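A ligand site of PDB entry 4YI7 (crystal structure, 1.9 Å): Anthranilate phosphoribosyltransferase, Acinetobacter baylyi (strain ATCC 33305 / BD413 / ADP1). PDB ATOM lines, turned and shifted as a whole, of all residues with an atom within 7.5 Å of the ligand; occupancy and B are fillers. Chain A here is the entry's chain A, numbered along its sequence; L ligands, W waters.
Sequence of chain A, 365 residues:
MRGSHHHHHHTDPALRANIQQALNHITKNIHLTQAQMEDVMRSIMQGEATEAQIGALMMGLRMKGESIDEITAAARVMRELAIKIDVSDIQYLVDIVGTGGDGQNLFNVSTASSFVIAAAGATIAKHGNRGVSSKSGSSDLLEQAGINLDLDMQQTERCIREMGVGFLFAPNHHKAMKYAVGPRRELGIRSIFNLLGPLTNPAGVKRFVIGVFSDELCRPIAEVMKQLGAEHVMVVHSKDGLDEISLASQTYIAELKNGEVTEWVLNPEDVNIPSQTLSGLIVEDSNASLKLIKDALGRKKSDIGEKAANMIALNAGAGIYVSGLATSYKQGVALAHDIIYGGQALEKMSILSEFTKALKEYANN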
ATOM      1  N   MET A  78       9.605 -29.732 -16.249  1.00  0.00           N
ATOM      2  CA  MET A  78       9.944 -28.477 -16.900  1.00  0.00           C
ATOM      3  C   MET A  78       8.714 -27.603 -17.094  1.00  0.00           C
ATOM      4  O   MET A  78       8.813 -26.382 -17.049  1.00  0.00           O
ATOM      5  CB  MET A  78      10.593 -28.726 -18.248  1.00  0.00           C
ATOM      6  CG  MET A  78      12.026 -29.206 -18.185  1.00  0.00           C
ATOM      7  SD  MET A  78      12.741 -29.301 -19.840  1.00  0.00           S
ATOM      8  CE  MET A  78      12.712 -27.590 -20.350  1.00  0.00           C
ATOM      9  N   ASP A  95       0.896 -25.644 -32.812  1.00  0.00           N
ATOM     10  CA  ASP A  95       2.297 -25.238 -32.650  1.00  0.00           C
ATOM     11  C   ASP A  95       3.122 -26.039 -33.632  1.00  0.00           C
ATOM     12  O   ASP A  95       2.844 -27.207 -33.838  1.00  0.00           O
ATOM     13  CB  ASP A  95       2.765 -25.473 -31.203  1.00  0.00           C
ATOM     14  CG  ASP A  95       4.209 -25.073 -30.952  1.00  0.00           C
ATOM     15  OD1 ASP A  95       4.844 -24.401 -31.813  1.00  0.00           O
ATOM     16  OD2 ASP A  95       4.716 -25.413 -29.865  1.00  0.00           O
ATOM     17  N   VAL A  97       7.087 -26.981 -34.382  1.00  0.00           N
ATOM     18  CA  VAL A  97       8.265 -26.936 -33.529  1.00  0.00           C
ATOM     19  C   VAL A  97       9.165 -28.159 -33.710  1.00  0.00           C
ATOM     20  O   VAL A  97       8.690 -29.274 -33.877  1.00  0.00           O
ATOM     21  CB  VAL A  97       7.843 -26.794 -32.056  1.00  0.00           C
ATOM     22  CG1 VAL A  97       7.052 -28.014 -31.594  1.00  0.00           C
ATOM     23  CG2 VAL A  97       9.076 -26.504 -31.161  1.00  0.00           C
ATOM     24  N   GLY A  98      10.477 -27.935 -33.661  1.00  0.00           N
ATOM     25  CA  GLY A  98      11.434 -29.000 -33.921  1.00  0.00           C
ATOM     26  C   GLY A  98      12.486 -29.088 -32.847  1.00  0.00           C
ATOM     27  O   GLY A  98      12.707 -28.131 -32.094  1.00  0.00           O
ATOM     28  N   THR A  99      13.138 -30.249 -32.769  1.00  0.00           N
ATOM     29  CA  THR A  99      14.202 -30.480 -31.807  1.00  0.00           C
ATOM     30  C   THR A  99      15.496 -29.793 -32.225  1.00  0.00           C
ATOM     31  O   THR A  99      16.380 -29.566 -31.401  1.00  0.00           O
ATOM     32  CB  THR A  99      14.511 -31.965 -31.660  1.00  0.00           C
ATOM     33  OG1 THR A  99      14.802 -32.499 -32.958  1.00  0.00           O
ATOM     34  CG2 THR A  99      13.343 -32.717 -31.031  1.00  0.00           C
ATOM     35  N   GLY A 100      15.573 -29.465 -33.511  1.00  0.00           N
ATOM     36  CA  GLY A 100      16.835 -29.279 -34.204  1.00  0.00           C
ATOM     37  C   GLY A 100      17.247 -30.589 -34.882  1.00  0.00           C
ATOM     38  O   GLY A 100      17.120 -31.663 -34.292  1.00  0.00           O
ATOM     39  N   LYS A 126       3.535 -20.319 -31.430  1.00  0.00           N
ATOM     40  CA  LYS A 126       4.740 -21.037 -31.808  1.00  0.00           C
ATOM     41  C   LYS A 126       5.803 -20.899 -30.737  1.00  0.00           C
ATOM     42  O   LYS A 126       6.267 -19.805 -30.423  1.00  0.00           O
ATOM     43  CB  LYS A 126       5.316 -20.562 -33.147  1.00  0.00           C
ATOM     44  CG  LYS A 126       6.567 -21.387 -33.530  1.00  0.00           C
ATOM     45  CD  LYS A 126       7.140 -21.072 -34.902  1.00  0.00           C
ATOM     46  CE  LYS A 126       8.593 -21.601 -35.017  1.00  0.00           C
ATOM     47  NZ  LYS A 126       8.918 -22.796 -34.131  1.00  0.00           N
ATOM     48  N   HIS A 127       6.168 -22.048 -30.206  1.00  0.00           N
ATOM     49  CA  HIS A 127       7.240 -22.169 -29.234  1.00  0.00           C
ATOM     50  C   HIS A 127       8.574 -22.175 -29.965  1.00  0.00           C
ATOM     51  O   HIS A 127       8.825 -23.041 -30.806  1.00  0.00           O
ATOM     52  CB  HIS A 127       7.034 -23.427 -28.422  1.00  0.00           C
ATOM     53  CG  HIS A 127       7.890 -23.516 -27.197  1.00  0.00           C
ATOM     54  ND1 HIS A 127       8.114 -24.689 -26.522  1.00  0.00           N
ATOM     55  CD2 HIS A 127       8.579 -22.557 -26.519  1.00  0.00           C
ATOM     56  CE1 HIS A 127       8.894 -24.456 -25.483  1.00  0.00           C
ATOM     57  NE2 HIS A 127       9.188 -23.177 -25.459  1.00  0.00           N
ATOM     58  N   GLY A 128       9.408 -21.188 -29.669  1.00  0.00           N
ATOM     59  CA  GLY A 128      10.682 -21.055 -30.361  1.00  0.00           C
ATOM     60  C   GLY A 128      11.837 -21.011 -29.389  1.00  0.00           C
ATOM     61  O   GLY A 128      11.649 -20.941 -28.172  1.00  0.00           O
ATOM     62  N   ASN A 129      13.036 -21.070 -29.932  1.00  0.00           N
ATOM     63  CA  ASN A 129      14.250 -21.002 -29.139  1.00  0.00           C
ATOM     64  C   ASN A 129      14.997 -19.716 -29.443  1.00  0.00           C
ATOM     65  O   ASN A 129      15.392 -19.473 -30.590  1.00  0.00           O
ATOM     66  CB  ASN A 129      15.116 -22.224 -29.408  1.00  0.00           C
ATOM     67  CG  ASN A 129      16.293 -22.305 -28.479  1.00  0.00           C
ATOM     68  OD1 ASN A 129      16.244 -21.826 -27.346  1.00  0.00           O
ATOM     69  ND2 ASN A 129      17.373 -22.924 -28.959  1.00  0.00           N
ATOM     70  N   ARG A 130      15.168 -18.879 -28.431  1.00  0.00           N
ATOM     71  CA  ARG A 130      15.826 -17.589 -28.587  1.00  0.00           C
ATOM     72  C   ARG A 130      17.352 -17.745 -28.558  1.00  0.00           C
ATOM     73  O   ARG A 130      17.903 -18.823 -28.777  1.00  0.00           O
ATOM     74  CB  ARG A 130      15.366 -16.617 -27.501  1.00  0.00           C
ATOM     75  N   LEU A 168       6.262 -17.604 -28.960  1.00  0.00           N
ATOM     76  CA  LEU A 168       6.624 -17.854 -27.573  1.00  0.00           C
ATOM     77  C   LEU A 168       8.096 -18.234 -27.416  1.00  0.00           C
ATOM     78  O   LEU A 168       8.501 -19.322 -27.829  1.00  0.00           O
ATOM     79  CB  LEU A 168       5.767 -18.963 -26.996  1.00  0.00           C
ATOM     80  CG  LEU A 168       4.254 -18.688 -27.031  1.00  0.00           C
ATOM     81  CD1 LEU A 168       3.498 -19.996 -26.934  1.00  0.00           C
ATOM     82  CD2 LEU A 168       3.879 -17.739 -25.910  1.00  0.00           C
ATOM     83  N   PHE A 169       8.872 -17.348 -26.807  1.00  0.00           N
ATOM     84  CA  PHE A 169      10.240 -17.655 -26.404  1.00  0.00           C
ATOM     85  C   PHE A 169      10.332 -17.673 -24.876  1.00  0.00           C
ATOM     86  O   PHE A 169       9.496 -17.066 -24.197  1.00  0.00           O
ATOM     87  CB  PHE A 169      11.221 -16.649 -26.996  1.00  0.00           C
ATOM     88  CG  PHE A 169      11.222 -16.605 -28.497  1.00  0.00           C
ATOM     89  CD1 PHE A 169      11.958 -17.521 -29.227  1.00  0.00           C
ATOM     90  CD2 PHE A 169      10.489 -15.648 -29.177  1.00  0.00           C
ATOM     91  CE1 PHE A 169      11.977 -17.487 -30.614  1.00  0.00           C
ATOM     92  CE2 PHE A 169      10.498 -15.610 -30.565  1.00  0.00           C
ATOM     93  CZ  PHE A 169      11.241 -16.530 -31.272  1.00  0.00           C
ATOM     94  N   ALA A 170      11.327 -18.372 -24.353  1.00  0.00           N
ATOM     95  CA  ALA A 170      11.517 -18.462 -22.901  1.00  0.00           C
ATOM     96  C   ALA A 170      11.790 -17.088 -22.300  1.00  0.00           C
ATOM     97  O   ALA A 170      11.337 -16.779 -21.188  1.00  0.00           O
ATOM     98  CB  ALA A 170      12.656 -19.435 -22.586  1.00  0.00           C
ATOM     99  N   MET A 177      16.201 -24.879 -19.114  1.00  0.00           N
ATOM    100  CA  MET A 177      16.453 -23.996 -17.976  1.00  0.00           C
ATOM    101  C   MET A 177      17.831 -23.351 -18.095  1.00  0.00           C
ATOM    102  O   MET A 177      18.514 -23.478 -19.111  1.00  0.00           O
ATOM    103  CB  MET A 177      16.346 -24.772 -16.663  1.00  0.00           C
ATOM    104  N   ARG A 184      24.880 -27.867 -22.737  1.00  0.00           N
ATOM    105  CA  ARG A 184      24.398 -28.127 -24.084  1.00  0.00           C
ATOM    106  C   ARG A 184      25.328 -27.555 -25.163  1.00  0.00           C
ATOM    107  O   ARG A 184      25.624 -28.223 -26.147  1.00  0.00           O
ATOM    108  CB  ARG A 184      22.983 -27.572 -24.266  1.00  0.00           C
ATOM    109  CG  ARG A 184      21.925 -28.378 -23.541  1.00  0.00           C
ATOM    110  CD  ARG A 184      20.531 -27.773 -23.739  1.00  0.00           C
ATOM    111  NE  ARG A 184      20.093 -27.929 -25.126  1.00  0.00           N
ATOM    112  CZ  ARG A 184      18.926 -27.502 -25.599  1.00  0.00           C
ATOM    113  NH1 ARG A 184      18.075 -26.875 -24.800  1.00  0.00           N
ATOM    114  NH2 ARG A 184      18.615 -27.689 -26.875  1.00  0.00           N
ATOM    115  N   SER A 191      20.280 -33.905 -27.549  1.00  0.00           N
ATOM    116  CA  SER A 191      20.049 -34.562 -26.270  1.00  0.00           C
ATOM    117  C   SER A 191      18.583 -34.488 -25.897  1.00  0.00           C
ATOM    118  O   SER A 191      17.767 -33.933 -26.623  1.00  0.00           O
ATOM    119  CB  SER A 191      20.887 -33.924 -25.157  1.00  0.00           C
ATOM    120  OG  SER A 191      20.363 -32.656 -24.804  1.00  0.00           O
ATOM    121  N   ILE A 192      18.266 -35.032 -24.726  1.00  0.00           N
ATOM    122  CA  ILE A 192      16.916 -34.974 -24.180  1.00  0.00           C
ATOM    123  C   ILE A 192      16.395 -33.530 -24.074  1.00  0.00           C
ATOM    124  O   ILE A 192      15.190 -33.285 -24.187  1.00  0.00           O
ATOM    125  CB  ILE A 192      16.861 -35.681 -22.808  1.00  0.00           C
ATOM    126  CG1 ILE A 192      15.405 -35.838 -22.327  1.00  0.00           C
ATOM    127  CG2 ILE A 192      17.689 -34.916 -21.763  1.00  0.00           C
ATOM    128  CD1 ILE A 192      15.253 -36.810 -21.190  1.00  0.00           C
ATOM    129  N   PHE A 193      17.281 -32.568 -23.867  1.00  0.00           N
ATOM    130  CA  PHE A 193      16.851 -31.164 -23.743  1.00  0.00           C
ATOM    131  C   PHE A 193      16.302 -30.622 -25.053  1.00  0.00           C
ATOM    132  O   PHE A 193      15.439 -29.741 -25.028  1.00  0.00           O
ATOM    133  CB  PHE A 193      17.989 -30.287 -23.255  1.00  0.00           C
ATOM    134  CG  PHE A 193      18.379 -30.540 -21.838  1.00  0.00           C
ATOM    135  CD1 PHE A 193      17.464 -30.342 -20.818  1.00  0.00           C
ATOM    136  CD2 PHE A 193      19.633 -31.003 -21.519  1.00  0.00           C
ATOM    137  CE1 PHE A 193      17.792 -30.587 -19.505  1.00  0.00           C
ATOM    138  CE2 PHE A 193      19.984 -31.242 -20.209  1.00  0.00           C
ATOM    139  CZ  PHE A 193      19.060 -31.044 -19.202  1.00  0.00           C
ATOM    140  N   ASN A 194      16.810 -31.129 -26.164  1.00  0.00           N
ATOM    141  CA  ASN A 194      16.235 -30.859 -27.487  1.00  0.00           C
ATOM    142  C   ASN A 194      14.835 -31.449 -27.600  1.00  0.00           C
ATOM    143  O   ASN A 194      13.916 -30.793 -28.088  1.00  0.00           O
ATOM    144  CB  ASN A 194      17.105 -31.457 -28.599  1.00  0.00           C
ATOM    145  CG  ASN A 194      18.486 -30.845 -28.641  1.00  0.00           C
ATOM    146  OD1 ASN A 194      19.364 -31.220 -27.868  1.00  0.00           O
ATOM    147  ND2 ASN A 194      18.684 -29.890 -29.544  1.00  0.00           N
ATOM    148  N   LEU A 195      14.693 -32.688 -27.150  1.00  0.00           N
ATOM    149  CA  LEU A 195      13.391 -33.356 -27.137  1.00  0.00           C
ATOM    150  C   LEU A 195      12.383 -32.568 -26.303  1.00  0.00           C
ATOM    151  O   LEU A 195      11.192 -32.539 -26.631  1.00  0.00           O
ATOM    152  CB  LEU A 195      13.521 -34.782 -26.575  1.00  0.00           C
ATOM    153  CG  LEU A 195      14.331 -35.805 -27.371  1.00  0.00           C
ATOM    154  CD1 LEU A 195      14.358 -37.114 -26.622  1.00  0.00           C
ATOM    155  CD2 LEU A 195      13.748 -36.006 -28.763  1.00  0.00           C
ATOM    156  N   LEU A 196      12.841 -31.925 -25.236  1.00  0.00           N
ATOM    157  CA  LEU A 196      11.934 -31.322 -24.281  1.00  0.00           C
ATOM    158  C   LEU A 196      11.391 -29.976 -24.766  1.00  0.00           C
ATOM    159  O   LEU A 196      10.358 -29.521 -24.295  1.00  0.00           O
ATOM    160  CB  LEU A 196      12.627 -31.150 -22.918  1.00  0.00           C
ATOM    161  CG  LEU A 196      12.795 -32.483 -22.164  1.00  0.00           C
ATOM    162  CD1 LEU A 196      13.790 -32.391 -21.019  1.00  0.00           C
ATOM    163  CD2 LEU A 196      11.474 -32.988 -21.653  1.00  0.00           C
ATOM    164  N   GLY A 197      12.081 -29.353 -25.716  1.00  0.00           N
ATOM    165  CA  GLY A 197      11.632 -28.083 -26.246  1.00  0.00           C
ATOM    166  C   GLY A 197      10.228 -28.179 -26.842  1.00  0.00           C
ATOM    167  O   GLY A 197       9.293 -27.493 -26.393  1.00  0.00           O
ATOM    168  N   PRO A 198      10.059 -29.060 -27.841  1.00  0.00           N
ATOM    169  CA  PRO A 198       8.714 -29.247 -28.397  1.00  0.00           C
ATOM    170  C   PRO A 198       7.659 -29.618 -27.347  1.00  0.00           C
ATOM    171  O   PRO A 198       6.497 -29.264 -27.487  1.00  0.00           O
ATOM    172  CB  PRO A 198       8.917 -30.395 -29.387  1.00  0.00           C
ATOM    173  CG  PRO A 198      10.345 -30.247 -29.835  1.00  0.00           C
ATOM    174  CD  PRO A 198      11.081 -29.819 -28.588  1.00  0.00           C
ATOM    175  N   LEU A 199       8.098 -30.290 -26.290  1.00  0.00           N
ATOM    176  CA  LEU A 199       7.202 -30.881 -25.301  1.00  0.00           C
ATOM    177  C   LEU A 199       6.820 -29.920 -24.177  1.00  0.00           C
ATOM    178  O   LEU A 199       6.081 -30.312 -23.266  1.00  0.00           O
ATOM    179  CB  LEU A 199       7.843 -32.138 -24.712  1.00  0.00           C
ATOM    180  CG  LEU A 199       7.642 -33.430 -25.518  1.00  0.00           C
ATOM    181  CD1 LEU A 199       7.946 -33.231 -26.997  1.00  0.00           C
ATOM    182  CD2 LEU A 199       8.497 -34.548 -24.938  1.00  0.00           C
ATOM    183  N   THR A 200       7.291 -28.675 -24.234  1.00  0.00           N
ATOM    184  CA  THR A 200       7.008 -27.695 -23.176  1.00  0.00           C
ATOM    185  C   THR A 200       6.445 -26.387 -23.708  1.00  0.00           C
ATOM    186  O   THR A 200       6.898 -25.306 -23.323  1.00  0.00           O
ATOM    187  CB  THR A 200       8.288 -27.386 -22.362  1.00  0.00           C
ATOM    188  OG1 THR A 200       9.295 -26.837 -23.214  1.00  0.00           O
ATOM    189  CG2 THR A 200       8.809 -28.663 -21.712  1.00  0.00           C
ATOM    190  N   ASN A 201       5.484 -26.468 -24.620  1.00  0.00           N
ATOM    191  CA  ASN A 201       4.767 -25.284 -25.038  1.00  0.00           C
ATOM    192  C   ASN A 201       4.112 -24.705 -23.784  1.00  0.00           C
ATOM    193  O   ASN A 201       3.492 -25.450 -23.034  1.00  0.00           O
ATOM    194  CB  ASN A 201       3.741 -25.616 -26.124  1.00  0.00           C
ATOM    195  CG  ASN A 201       3.012 -24.396 -26.618  1.00  0.00           C
ATOM    196  OD1 ASN A 201       2.224 -23.794 -25.894  1.00  0.00           O
ATOM    197  ND2 ASN A 201       3.265 -24.015 -27.864  1.00  0.00           N
ATOM    198  N   GLY A 211       9.130 -31.835 -35.140  1.00  0.00           N
ATOM    199  CA  GLY A 211      10.259 -32.432 -35.813  1.00  0.00           C
ATOM    200  C   GLY A 211      11.280 -32.968 -34.816  1.00  0.00           C
ATOM    201  O   GLY A 211      11.565 -32.341 -33.793  1.00  0.00           O
ATOM    202  N   ASP A 243      14.569 -32.141 -39.226  1.00  0.00           N
ATOM    203  CA  ASP A 243      13.509 -32.194 -38.230  1.00  0.00           C
ATOM    204  C   ASP A 243      12.301 -31.475 -38.813  1.00  0.00           C
ATOM    205  O   ASP A 243      11.661 -30.639 -38.164  1.00  0.00           O
ATOM    206  CB  ASP A 243      13.943 -31.576 -36.895  1.00  0.00           C
ATOM    207  CG  ASP A 243      14.273 -30.091 -37.002  1.00  0.00           C
ATOM    208  OD1 ASP A 243      14.624 -29.610 -38.103  1.00  0.00           O
ATOM    209  OD2 ASP A 243      14.171 -29.407 -35.967  1.00  0.00           O
HETATM  210  C1  LIG L   1      15.443 -26.225 -27.209  1.00  0.00           C
HETATM  211  O1  LIG L   1      16.192 -26.957 -27.915  1.00  0.00           O
HETATM  212  O2  LIG L   1      15.846 -25.856 -26.072  1.00  0.00           O
HETATM  213  C2  LIG L   1      14.076 -25.799 -27.715  1.00  0.00           C
HETATM  214  C3  LIG L   1      13.582 -26.334 -28.889  1.00  0.00           C
HETATM  215  C4  LIG L   1      12.322 -25.954 -29.353  1.00  0.00           C
HETATM  216  N1  LIG L   1      14.348 -27.261 -29.639  1.00  0.00           N
HETATM  217  C5  LIG L   1      11.562 -25.043 -28.620  1.00  0.00           C
HETATM  218  C6  LIG L   1      12.063 -24.516 -27.437  1.00  0.00           C
HETATM  219  C7  LIG L   1      13.325 -24.892 -26.982  1.00  0.00           C
HETATM  220  O   HOH W   1      14.314 -27.691 -24.098  1.00  0.00           O
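The guanidinium group (NH2) of Arg 184 sits close to the side-chain amide nitrogen (ND2) of Asn 194 (3.5 Å). The backbone carbonyl oxygen of Thr 99 lies within hydrogen-bond range of the side-chain amide nitrogen of Asn 194, 3.0 Å away. N of Thr 99 is in hydrogen-bond range of OD2 of Asp 243 (3.5 Å). The backbone NH (N) of Thr 99 sits at hydrogen-bond distance from the backbone carbonyl oxygen (O) of Gly 211, 2.8 Å away. OG1 of Thr 200 sits at hydrogen-bond distance from O of Gly 197, at 3.2 Å. The backbone carbonyl oxygen (O) of Leu 168 lies within hydrogen-bond range of the backbone NH (N) of Gly 128. ND1 of His 127 sits close to O of Thr 200, at 3.5 Å. The side-chain carboxylate (OD1) of Asp 95 sits at hydrogen-bond distance from the backbone NH (N) of His 127, at 3.1 Å.
Water W1 lies within hydrogen-bond range of the backbone carbonyl oxygen (O) of Phe 193, an oxygen (O2) of the ligand and the backbone NH (N) of Gly 197.
Val 97 touches the ligand (CG2 to C4, 3.8 Å). Thr 99 touches the ligand. CE1 of His 127 touches C6 of the ligand, at 3.7 Å. Gly 128 touches the ligand. O of Asn 194 touches N1 of the ligand (3.9 Å). Gly 197 touches the ligand. Within 4 Å of the ligand: Val 97, Gly 98, Thr 99, His 127, Gly 128, Arg 184, Asn 194 and Gly 197. The nearest printed residue that does not touch the ligand is Asn 129 (4.03 Å).
NH2 of Arg 184 lies within salt-bridge range of O1 of the ligand. O of Gly 98 lies within hydrogen-bond range of N1 of the ligand (3.1 Å).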
